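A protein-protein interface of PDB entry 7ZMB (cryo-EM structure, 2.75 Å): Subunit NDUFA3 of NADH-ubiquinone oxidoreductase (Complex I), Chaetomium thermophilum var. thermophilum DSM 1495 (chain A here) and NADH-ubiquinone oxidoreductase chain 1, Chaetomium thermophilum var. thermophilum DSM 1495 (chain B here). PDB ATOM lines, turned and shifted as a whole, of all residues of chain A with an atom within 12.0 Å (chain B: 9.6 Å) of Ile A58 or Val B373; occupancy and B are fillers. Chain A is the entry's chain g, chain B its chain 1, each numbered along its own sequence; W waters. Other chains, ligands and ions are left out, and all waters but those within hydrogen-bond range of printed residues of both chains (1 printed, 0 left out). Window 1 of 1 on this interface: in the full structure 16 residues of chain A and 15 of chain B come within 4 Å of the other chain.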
ATOM      1  N   VAL A  53     -15.148  -0.150 -34.176  1.00  0.00           N
ATOM      2  CA  VAL A  53     -14.000   0.299 -33.338  1.00  0.00           C
ATOM      3  C   VAL A  53     -14.483   0.621 -31.927  1.00  0.00           C
ATOM      4  O   VAL A  53     -15.471   1.360 -31.796  1.00  0.00           O
ATOM      5  CB  VAL A  53     -13.280   1.497 -33.987  1.00  0.00           C
ATOM      6  CG1 VAL A  53     -12.170   2.046 -33.105  1.00  0.00           C
ATOM      7  CG2 VAL A  53     -12.736   1.151 -35.363  1.00  0.00           C
ATOM      8  N   ASP A  54     -13.802   0.077 -30.917  1.00  0.00           N
ATOM      9  CA  ASP A  54     -14.130   0.414 -29.509  1.00  0.00           C
ATOM     10  C   ASP A  54     -13.935   1.926 -29.369  1.00  0.00           C
ATOM     11  O   ASP A  54     -12.933   2.441 -29.889  1.00  0.00           O
ATOM     12  CB  ASP A  54     -13.224  -0.405 -28.584  1.00  0.00           C
ATOM     13  CG  ASP A  54     -13.260  -0.086 -27.098  1.00  0.00           C
ATOM     14  OD1 ASP A  54     -12.559  -0.783 -26.342  1.00  0.00           O
ATOM     15  OD2 ASP A  54     -13.978   0.842 -26.699  1.00  0.00           O
ATOM     16  N   ALA A  55     -14.861   2.606 -28.691  1.00  0.00           N
ATOM     17  CA  ALA A  55     -14.783   4.076 -28.558  1.00  0.00           C
ATOM     18  C   ALA A  55     -13.670   4.468 -27.589  1.00  0.00           C
ATOM     19  O   ALA A  55     -13.246   3.611 -26.795  1.00  0.00           O
ATOM     20  CB  ALA A  55     -16.117   4.632 -28.143  1.00  0.00           C
ATOM     21  N   ALA A  56     -13.205   5.713 -27.674  1.00  0.00           N
ATOM     22  CA  ALA A  56     -12.173   6.211 -26.735  1.00  0.00           C
ATOM     23  C   ALA A  56     -12.768   6.385 -25.328  1.00  0.00           C
ATOM     24  O   ALA A  56     -13.964   6.716 -25.251  1.00  0.00           O
ATOM     25  CB  ALA A  56     -11.612   7.508 -27.243  1.00  0.00           C
ATOM     26  N   PRO A  57     -12.031   6.176 -24.204  1.00  0.00           N
ATOM     27  CA  PRO A  57     -12.616   6.445 -22.892  1.00  0.00           C
ATOM     28  C   PRO A  57     -13.021   7.920 -22.709  1.00  0.00           C
ATOM     29  O   PRO A  57     -12.259   8.788 -23.071  1.00  0.00           O
ATOM     30  CB  PRO A  57     -11.480   6.056 -21.940  1.00  0.00           C
ATOM     31  CG  PRO A  57     -10.229   6.179 -22.774  1.00  0.00           C
ATOM     32  CD  PRO A  57     -10.656   5.688 -24.138  1.00  0.00           C
ATOM     33  N   ILE A  58     -14.203   8.163 -22.137  1.00  0.00           N
ATOM     34  CA  ILE A  58     -14.703   9.555 -21.910  1.00  0.00           C
ATOM     35  C   ILE A  58     -13.909  10.220 -20.776  1.00  0.00           C
ATOM     36  O   ILE A  58     -13.486   9.507 -19.856  1.00  0.00           O
ATOM     37  CB  ILE A  58     -16.224   9.568 -21.673  1.00  0.00           C
ATOM     38  CG1 ILE A  58     -16.607   9.013 -20.299  1.00  0.00           C
ATOM     39  CG2 ILE A  58     -16.945   8.848 -22.800  1.00  0.00           C
ATOM     40  CD1 ILE A  58     -17.726   9.769 -19.630  1.00  0.00           C
ATOM     41  N   PRO A  59     -13.636  11.539 -20.821  1.00  0.00           N
ATOM     42  CA  PRO A  59     -12.819  12.175 -19.782  1.00  0.00           C
ATOM     43  C   PRO A  59     -13.524  12.165 -18.410  1.00  0.00           C
ATOM     44  O   PRO A  59     -14.676  12.513 -18.344  1.00  0.00           O
ATOM     45  CB  PRO A  59     -12.585  13.582 -20.351  1.00  0.00           C
ATOM     46  CG  PRO A  59     -13.737  13.820 -21.297  1.00  0.00           C
ATOM     47  CD  PRO A  59     -14.056  12.459 -21.875  1.00  0.00           C
ATOM     48  N   LEU A  60     -12.830  11.735 -17.358  1.00  0.00           N
ATOM     49  CA  LEU A  60     -13.431  11.651 -16.001  1.00  0.00           C
ATOM     50  C   LEU A  60     -12.586  12.508 -15.069  1.00  0.00           C
ATOM     51  O   LEU A  60     -13.028  12.750 -13.940  1.00  0.00           O
ATOM     52  CB  LEU A  60     -13.537  10.187 -15.570  1.00  0.00           C
ATOM     53  CG  LEU A  60     -14.525   9.342 -16.373  1.00  0.00           C
ATOM     54  CD1 LEU A  60     -14.621   7.934 -15.818  1.00  0.00           C
ATOM     55  CD2 LEU A  60     -15.895   9.994 -16.386  1.00  0.00           C
ATOM     56  N   THR A  61     -11.509  13.081 -15.590  1.00  0.00           N
ATOM     57  CA  THR A  61     -10.699  14.066 -14.831  1.00  0.00           C
ATOM     58  C   THR A  61     -10.229  15.074 -15.878  1.00  0.00           C
ATOM     59  O   THR A  61     -10.254  14.729 -17.069  1.00  0.00           O
ATOM     60  CB  THR A  61      -9.485  13.418 -14.150  1.00  0.00           C
ATOM     61  OG1 THR A  61      -8.893  14.361 -13.259  1.00  0.00           O
ATOM     62  CG2 THR A  61      -8.441  12.932 -15.131  1.00  0.00           C
ATOM     63  N   TYR A  62      -9.959  16.310 -15.465  1.00  0.00           N
ATOM     64  CA  TYR A  62      -9.475  17.331 -16.423  1.00  0.00           C
ATOM     65  C   TYR A  62      -8.243  16.754 -17.119  1.00  0.00           C
ATOM     66  O   TYR A  62      -7.340  16.239 -16.447  1.00  0.00           O
ATOM     67  CB  TYR A  62      -9.142  18.648 -15.719  1.00  0.00           C
ATOM     68  CG  TYR A  62      -8.906  19.813 -16.648  1.00  0.00           C
ATOM     69  CD1 TYR A  62      -7.691  19.990 -17.289  1.00  0.00           C
ATOM     70  CD2 TYR A  62      -9.903  20.743 -16.889  1.00  0.00           C
ATOM     71  CE1 TYR A  62      -7.474  21.047 -18.156  1.00  0.00           C
ATOM     72  CE2 TYR A  62      -9.699  21.813 -17.742  1.00  0.00           C
ATOM     73  CZ  TYR A  62      -8.482  21.964 -18.381  1.00  0.00           C
ATOM     74  OH  TYR A  62      -8.286  23.022 -19.218  1.00  0.00           O
ATOM     75  N   PRO A  63      -8.173  16.831 -18.460  1.00  0.00           N
ATOM     76  CA  PRO A  63      -7.048  16.276 -19.184  1.00  0.00           C
ATOM     77  C   PRO A  63      -5.942  17.332 -19.137  1.00  0.00           C
ATOM     78  O   PRO A  63      -6.025  18.302 -19.845  1.00  0.00           O
ATOM     79  CB  PRO A  63      -7.585  16.128 -20.614  1.00  0.00           C
ATOM     80  CG  PRO A  63      -9.063  16.450 -20.527  1.00  0.00           C
ATOM     81  CD  PRO A  63      -9.198  17.377 -19.342  1.00  0.00           C
ATOM     82  N   ILE A  64      -4.941  17.099 -18.297  1.00  0.00           N
ATOM     83  CA  ILE A  64      -3.840  18.089 -18.163  1.00  0.00           C
ATOM     84  C   ILE A  64      -2.963  17.938 -19.405  1.00  0.00           C
ATOM     85  O   ILE A  64      -2.503  16.808 -19.635  1.00  0.00           O
ATOM     86  CB  ILE A  64      -3.047  17.947 -16.850  1.00  0.00           C
ATOM     87  CG1 ILE A  64      -3.939  18.131 -15.621  1.00  0.00           C
ATOM     88  CG2 ILE A  64      -1.865  18.901 -16.839  1.00  0.00           C
ATOM     89  CD1 ILE A  64      -4.327  19.562 -15.362  1.00  0.00           C
ATOM     90  N   ILE B 163     -29.422  -3.456 -13.533  1.00  0.00           N
ATOM     91  CA  ILE B 163     -28.401  -2.443 -13.154  1.00  0.00           C
ATOM     92  C   ILE B 163     -27.191  -2.546 -14.090  1.00  0.00           C
ATOM     93  O   ILE B 163     -26.598  -1.513 -14.387  1.00  0.00           O
ATOM     94  CB  ILE B 163     -28.038  -2.536 -11.661  1.00  0.00           C
ATOM     95  CG1 ILE B 163     -29.236  -2.948 -10.800  1.00  0.00           C
ATOM     96  CG2 ILE B 163     -27.409  -1.237 -11.185  1.00  0.00           C
ATOM     97  CD1 ILE B 163     -30.400  -1.982 -10.834  1.00  0.00           C
ATOM     98  N   MET B 164     -26.847  -3.746 -14.545  1.00  0.00           N
ATOM     99  CA  MET B 164     -25.737  -3.874 -15.517  1.00  0.00           C
ATOM    100  C   MET B 164     -26.066  -3.076 -16.785  1.00  0.00           C
ATOM    101  O   MET B 164     -25.166  -2.402 -17.285  1.00  0.00           O
ATOM    102  CB  MET B 164     -25.442  -5.338 -15.826  1.00  0.00           C
ATOM    103  CG  MET B 164     -24.900  -6.099 -14.635  1.00  0.00           C
ATOM    104  SD  MET B 164     -24.911  -7.886 -14.899  1.00  0.00           S
ATOM    105  CE  MET B 164     -24.081  -8.454 -13.415  1.00  0.00           C
ATOM    106  N   LEU B 165     -27.300  -3.147 -17.297  1.00  0.00           N
ATOM    107  CA  LEU B 165     -27.664  -2.287 -18.458  1.00  0.00           C
ATOM    108  C   LEU B 165     -27.753  -0.802 -18.086  1.00  0.00           C
ATOM    109  O   LEU B 165     -27.203  -0.004 -18.841  1.00  0.00           O
ATOM    110  CB  LEU B 165     -28.990  -2.757 -19.059  1.00  0.00           C
ATOM    111  CG  LEU B 165     -29.061  -4.208 -19.526  1.00  0.00           C
ATOM    112  CD1 LEU B 165     -30.259  -4.395 -20.440  1.00  0.00           C
ATOM    113  CD2 LEU B 165     -27.786  -4.616 -20.242  1.00  0.00           C
ATOM    114  N   SER B 166     -28.451  -0.440 -17.005  1.00  0.00           N
ATOM    115  CA  SER B 166     -28.664   0.994 -16.648  1.00  0.00           C
ATOM    116  C   SER B 166     -27.398   1.647 -16.095  1.00  0.00           C
ATOM    117  O   SER B 166     -27.111   2.780 -16.494  1.00  0.00           O
ATOM    118  CB  SER B 166     -29.818   1.148 -15.707  1.00  0.00           C
ATOM    119  OG  SER B 166     -29.527   0.579 -14.440  1.00  0.00           O
ATOM    120  N   GLY B 167     -26.706   0.956 -15.187  1.00  0.00           N
ATOM    121  CA  GLY B 167     -25.478   1.463 -14.553  1.00  0.00           C
ATOM    122  C   GLY B 167     -25.793   2.427 -13.433  1.00  0.00           C
ATOM    123  O   GLY B 167     -24.857   3.083 -12.954  1.00  0.00           O
ATOM    124  N   SER B 168     -27.055   2.499 -12.998  1.00  0.00           N
ATOM    125  CA  SER B 168     -27.375   3.580 -12.035  1.00  0.00           C
ATOM    126  C   SER B 168     -27.838   3.193 -10.640  1.00  0.00           C
ATOM    127  O   SER B 168     -27.234   3.771  -9.707  1.00  0.00           O
ATOM    128  CB  SER B 168     -28.276   4.592 -12.626  1.00  0.00           C
ATOM    129  OG  SER B 168     -28.543   5.615 -11.687  1.00  0.00           O
ATOM    130  N   LEU B 169     -28.857   2.347 -10.489  1.00  0.00           N
ATOM    131  CA  LEU B 169     -29.478   2.099  -9.146  1.00  0.00           C
ATOM    132  C   LEU B 169     -30.467   3.232  -8.804  1.00  0.00           C
ATOM    133  O   LEU B 169     -31.114   3.128  -7.767  1.00  0.00           O
ATOM    134  CB  LEU B 169     -28.463   1.870  -8.014  1.00  0.00           C
ATOM    135  CG  LEU B 169     -28.012   0.431  -7.781  1.00  0.00           C
ATOM    136  CD1 LEU B 169     -27.159   0.340  -6.530  1.00  0.00           C
ATOM    137  CD2 LEU B 169     -29.207  -0.498  -7.662  1.00  0.00           C
ATOM    138  N   VAL B 173     -33.214   7.079 -13.699  1.00  0.00           N
ATOM    139  CA  VAL B 173     -32.150   6.846 -14.715  1.00  0.00           C
ATOM    140  C   VAL B 173     -32.459   5.564 -15.483  1.00  0.00           C
ATOM    141  O   VAL B 173     -32.251   5.544 -16.693  1.00  0.00           O
ATOM    142  CB  VAL B 173     -30.743   6.836 -14.088  1.00  0.00           C
ATOM    143  CG1 VAL B 173     -29.669   6.580 -15.131  1.00  0.00           C
ATOM    144  CG2 VAL B 173     -30.454   8.122 -13.335  1.00  0.00           C
ATOM    145  N   SER B 177     -32.998   5.399 -19.375  1.00  0.00           N
ATOM    146  CA  SER B 177     -32.168   4.487 -20.205  1.00  0.00           C
ATOM    147  C   SER B 177     -33.056   3.713 -21.188  1.00  0.00           C
ATOM    148  O   SER B 177     -32.587   3.432 -22.291  1.00  0.00           O
ATOM    149  CB  SER B 177     -31.332   3.584 -19.329  1.00  0.00           C
ATOM    150  OG  SER B 177     -30.486   4.337 -18.480  1.00  0.00           O
ATOM    151  N   LEU B 365     -21.905  -7.242 -23.062  1.00  0.00           N
ATOM    152  CA  LEU B 365     -21.685  -5.773 -22.960  1.00  0.00           C
ATOM    153  C   LEU B 365     -20.250  -5.381 -23.340  1.00  0.00           C
ATOM    154  O   LEU B 365     -20.102  -4.499 -24.189  1.00  0.00           O
ATOM    155  CB  LEU B 365     -22.029  -5.323 -21.541  1.00  0.00           C
ATOM    156  CG  LEU B 365     -23.478  -5.525 -21.099  1.00  0.00           C
ATOM    157  CD1 LEU B 365     -23.679  -5.052 -19.669  1.00  0.00           C
ATOM    158  CD2 LEU B 365     -24.441  -4.816 -22.030  1.00  0.00           C
ATOM    159  N   ASN B 369     -18.924  -3.335 -26.758  1.00  0.00           N
ATOM    160  CA  ASN B 369     -18.523  -1.987 -26.277  1.00  0.00           C
ATOM    161  C   ASN B 369     -19.736  -1.239 -25.720  1.00  0.00           C
ATOM    162  O   ASN B 369     -19.830  -0.029 -25.953  1.00  0.00           O
ATOM    163  CB  ASN B 369     -17.817  -1.166 -27.357  1.00  0.00           C
ATOM    164  CG  ASN B 369     -16.929  -0.088 -26.782  1.00  0.00           C
ATOM    165  OD1 ASN B 369     -16.836   1.004 -27.335  1.00  0.00           O
ATOM    166  ND2 ASN B 369     -16.294  -0.380 -25.660  1.00  0.00           N
ATOM    167  N   ILE B 370     -20.638  -1.937 -25.030  1.00  0.00           N
ATOM    168  CA  ILE B 370     -21.869  -1.257 -24.538  1.00  0.00           C
ATOM    169  C   ILE B 370     -21.972  -1.250 -23.013  1.00  0.00           C
ATOM    170  O   ILE B 370     -23.094  -1.416 -22.515  1.00  0.00           O
ATOM    171  CB  ILE B 370     -23.148  -1.741 -25.259  1.00  0.00           C
ATOM    172  CG1 ILE B 370     -23.298  -3.262 -25.225  1.00  0.00           C
ATOM    173  CG2 ILE B 370     -23.179  -1.207 -26.680  1.00  0.00           C
ATOM    174  CD1 ILE B 370     -24.708  -3.731 -25.465  1.00  0.00           C
ATOM    175  N   PHE B 371     -20.864  -1.067 -22.299  1.00  0.00           N
ATOM    176  CA  PHE B 371     -20.973  -0.875 -20.829  1.00  0.00           C
ATOM    177  C   PHE B 371     -21.457   0.565 -20.650  1.00  0.00           C
ATOM    178  O   PHE B 371     -20.860   1.482 -21.234  1.00  0.00           O
ATOM    179  CB  PHE B 371     -19.642  -1.042 -20.092  1.00  0.00           C
ATOM    180  CG  PHE B 371     -19.212  -2.447 -19.759  1.00  0.00           C
ATOM    181  CD1 PHE B 371     -20.123  -3.390 -19.317  1.00  0.00           C
ATOM    182  CD2 PHE B 371     -17.878  -2.809 -19.834  1.00  0.00           C
ATOM    183  CE1 PHE B 371     -19.713  -4.672 -18.988  1.00  0.00           C
ATOM    184  CE2 PHE B 371     -17.469  -4.090 -19.504  1.00  0.00           C
ATOM    185  CZ  PHE B 371     -18.388  -5.020 -19.083  1.00  0.00           C
ATOM    186  N   PRO B 372     -22.536   0.810 -19.887  1.00  0.00           N
ATOM    187  CA  PRO B 372     -22.997   2.168 -19.660  1.00  0.00           C
ATOM    188  C   PRO B 372     -22.042   3.010 -18.807  1.00  0.00           C
ATOM    189  O   PRO B 372     -21.474   2.486 -17.884  1.00  0.00           O
ATOM    190  CB  PRO B 372     -24.323   1.938 -18.922  1.00  0.00           C
ATOM    191  CG  PRO B 372     -24.121   0.628 -18.210  1.00  0.00           C
ATOM    192  CD  PRO B 372     -23.341  -0.202 -19.203  1.00  0.00           C
ATOM    193  N   VAL B 373     -21.897   4.291 -19.137  1.00  0.00           N
ATOM    194  CA  VAL B 373     -21.104   5.202 -18.268  1.00  0.00           C
ATOM    195  C   VAL B 373     -21.855   5.275 -16.935  1.00  0.00           C
ATOM    196  O   VAL B 373     -23.095   5.280 -16.955  1.00  0.00           O
ATOM    197  CB  VAL B 373     -20.849   6.582 -18.902  1.00  0.00           C
ATOM    198  CG1 VAL B 373     -19.883   6.514 -20.069  1.00  0.00           C
ATOM    199  CG2 VAL B 373     -22.137   7.267 -19.316  1.00  0.00           C
ATOM    200  N   ASN B 374     -21.137   5.292 -15.821  1.00  0.00           N
ATOM    201  CA  ASN B 374     -21.811   5.207 -14.498  1.00  0.00           C
ATOM    202  C   ASN B 374     -21.854   6.598 -13.865  1.00  0.00           C
ATOM    203  O   ASN B 374     -22.139   6.697 -12.671  1.00  0.00           O
ATOM    204  CB  ASN B 374     -21.161   4.091 -13.679  1.00  0.00           C
ATOM    205  CG  ASN B 374     -21.196   2.751 -14.380  1.00  0.00           C
ATOM    206  OD1 ASN B 374     -20.180   2.264 -14.859  1.00  0.00           O
ATOM    207  ND2 ASN B 374     -22.367   2.149 -14.458  1.00  0.00           N
ATOM    208  N   ILE B 375     -21.606   7.624 -14.668  1.00  0.00           N
ATOM    209  CA  ILE B 375     -21.673   9.037 -14.205  1.00  0.00           C
ATOM    210  C   ILE B 375     -23.142   9.454 -14.181  1.00  0.00           C
ATOM    211  O   ILE B 375     -23.984   8.682 -14.664  1.00  0.00           O
ATOM    212  CB  ILE B 375     -20.859   9.920 -15.174  1.00  0.00           C
ATOM    213  CG1 ILE B 375     -21.516  10.023 -16.551  1.00  0.00           C
ATOM    214  CG2 ILE B 375     -19.420   9.438 -15.268  1.00  0.00           C
ATOM    215  CD1 ILE B 375     -20.876  11.048 -17.454  1.00  0.00           C
ATOM    216  N   SER B 376     -23.430  10.653 -13.680  1.00  0.00           N
ATOM    217  CA  SER B 376     -24.818  11.168 -13.739  1.00  0.00           C
ATOM    218  C   SER B 376     -25.027  11.771 -15.129  1.00  0.00           C
ATOM    219  O   SER B 376     -24.231  12.626 -15.520  1.00  0.00           O
ATOM    220  CB  SER B 376     -25.059  12.163 -12.649  1.00  0.00           C
ATOM    221  OG  SER B 376     -24.628  11.649 -11.400  1.00  0.00           O
ATOM    222  N   LEU B 377     -26.019  11.280 -15.864  1.00  0.00           N
ATOM    223  CA  LEU B 377     -26.286  11.773 -17.240  1.00  0.00           C
ATOM    224  C   LEU B 377     -27.795  11.881 -17.428  1.00  0.00           C
ATOM    225  O   LEU B 377     -28.290  13.003 -17.630  1.00  0.00           O
ATOM    226  CB  LEU B 377     -25.665  10.799 -18.244  1.00  0.00           C
ATOM    227  CG  LEU B 377     -25.882  11.126 -19.719  1.00  0.00           C
ATOM    228  CD1 LEU B 377     -25.032  12.311 -20.145  1.00  0.00           C
ATOM    229  CD2 LEU B 377     -25.577   9.912 -20.580  1.00  0.00           C
ATOM    230  N   LEU B 378     -28.487  10.745 -17.380  1.00  0.00           N
ATOM    231  CA  LEU B 378     -29.953  10.733 -17.603  1.00  0.00           C
ATOM    232  C   LEU B 378     -30.659  10.782 -16.239  1.00  0.00           C
ATOM    233  O   LEU B 378     -31.398  11.745 -16.015  1.00  0.00           O
ATOM    234  CB  LEU B 378     -30.294   9.441 -18.354  1.00  0.00           C
ATOM    235  CG  LEU B 378     -29.509   9.178 -19.637  1.00  0.00           C
ATOM    236  CD1 LEU B 378     -29.740   7.758 -20.125  1.00  0.00           C
ATOM    237  CD2 LEU B 378     -29.893  10.170 -20.718  1.00  0.00           C
HETATM  238  O   HOH W   1     -15.409   2.349 -24.799  1.00  0.00           O
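Water W1 lies within hydrogen-bond range of OD2 of Asp A54 (2.8 Å), ND2 of Asn B369 (3.0 Å) and O of Ala A55 (3.2 Å).
Val B373 touches Ile A58 (CG1 to CD1, 3.9 Å).
CG2 of Ile B375 touches CD2 of Leu A60, at 3.7 Å.
Printed residues of chain B within 4 Å of Asp A54: Asn B369 (2.8 Å).
Of the printed residues of chain B, Ala A55 touches Asn B369 (2.9 Å).
No residue of chain B comes within 4 Å of Pro A57.
Ile A58 touches one residue of chain B.
No residue of chain B comes within 4 Å of Pro A59.
Of the printed residues of chain B, Leu A60 touches Ile B375 (3.7 Å).
No residue of chain A comes within 4 Å of Gly B167.
Leu B365 touches none of the printed residues of chain A.
Of the printed residues of chain A, Asn B369 touches Asp A54 and Ala A55.
No residue of chain A comes within 4 Å of Pro B372.
Val B373 touches just one residue of chain A: Ile A58.
No residue of chain A comes within 4 Å of Asn B374.
The nearest residue of chain B that does not touch Ile A58 is Ile B375 (4.04 Å).
The nearest printed residue of chain A that does not touch Asn B369 is Val A53 (4.7 Å).
ND2 of Asn B369 is in hydrogen-bond range of OD2 of Asp A54, 2.8 Å away.
The side-chain amide oxygen (OD1) of Asn B369 is in hydrogen-bond range of the backbone NH (N) of Ala A55.
Of the 12 printed residues of chain A, 4 touch a printed residue of chain B.
Printed residues of chain B that touch a printed residue of chain A: Asn B369, Val B373 and Ile B375.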
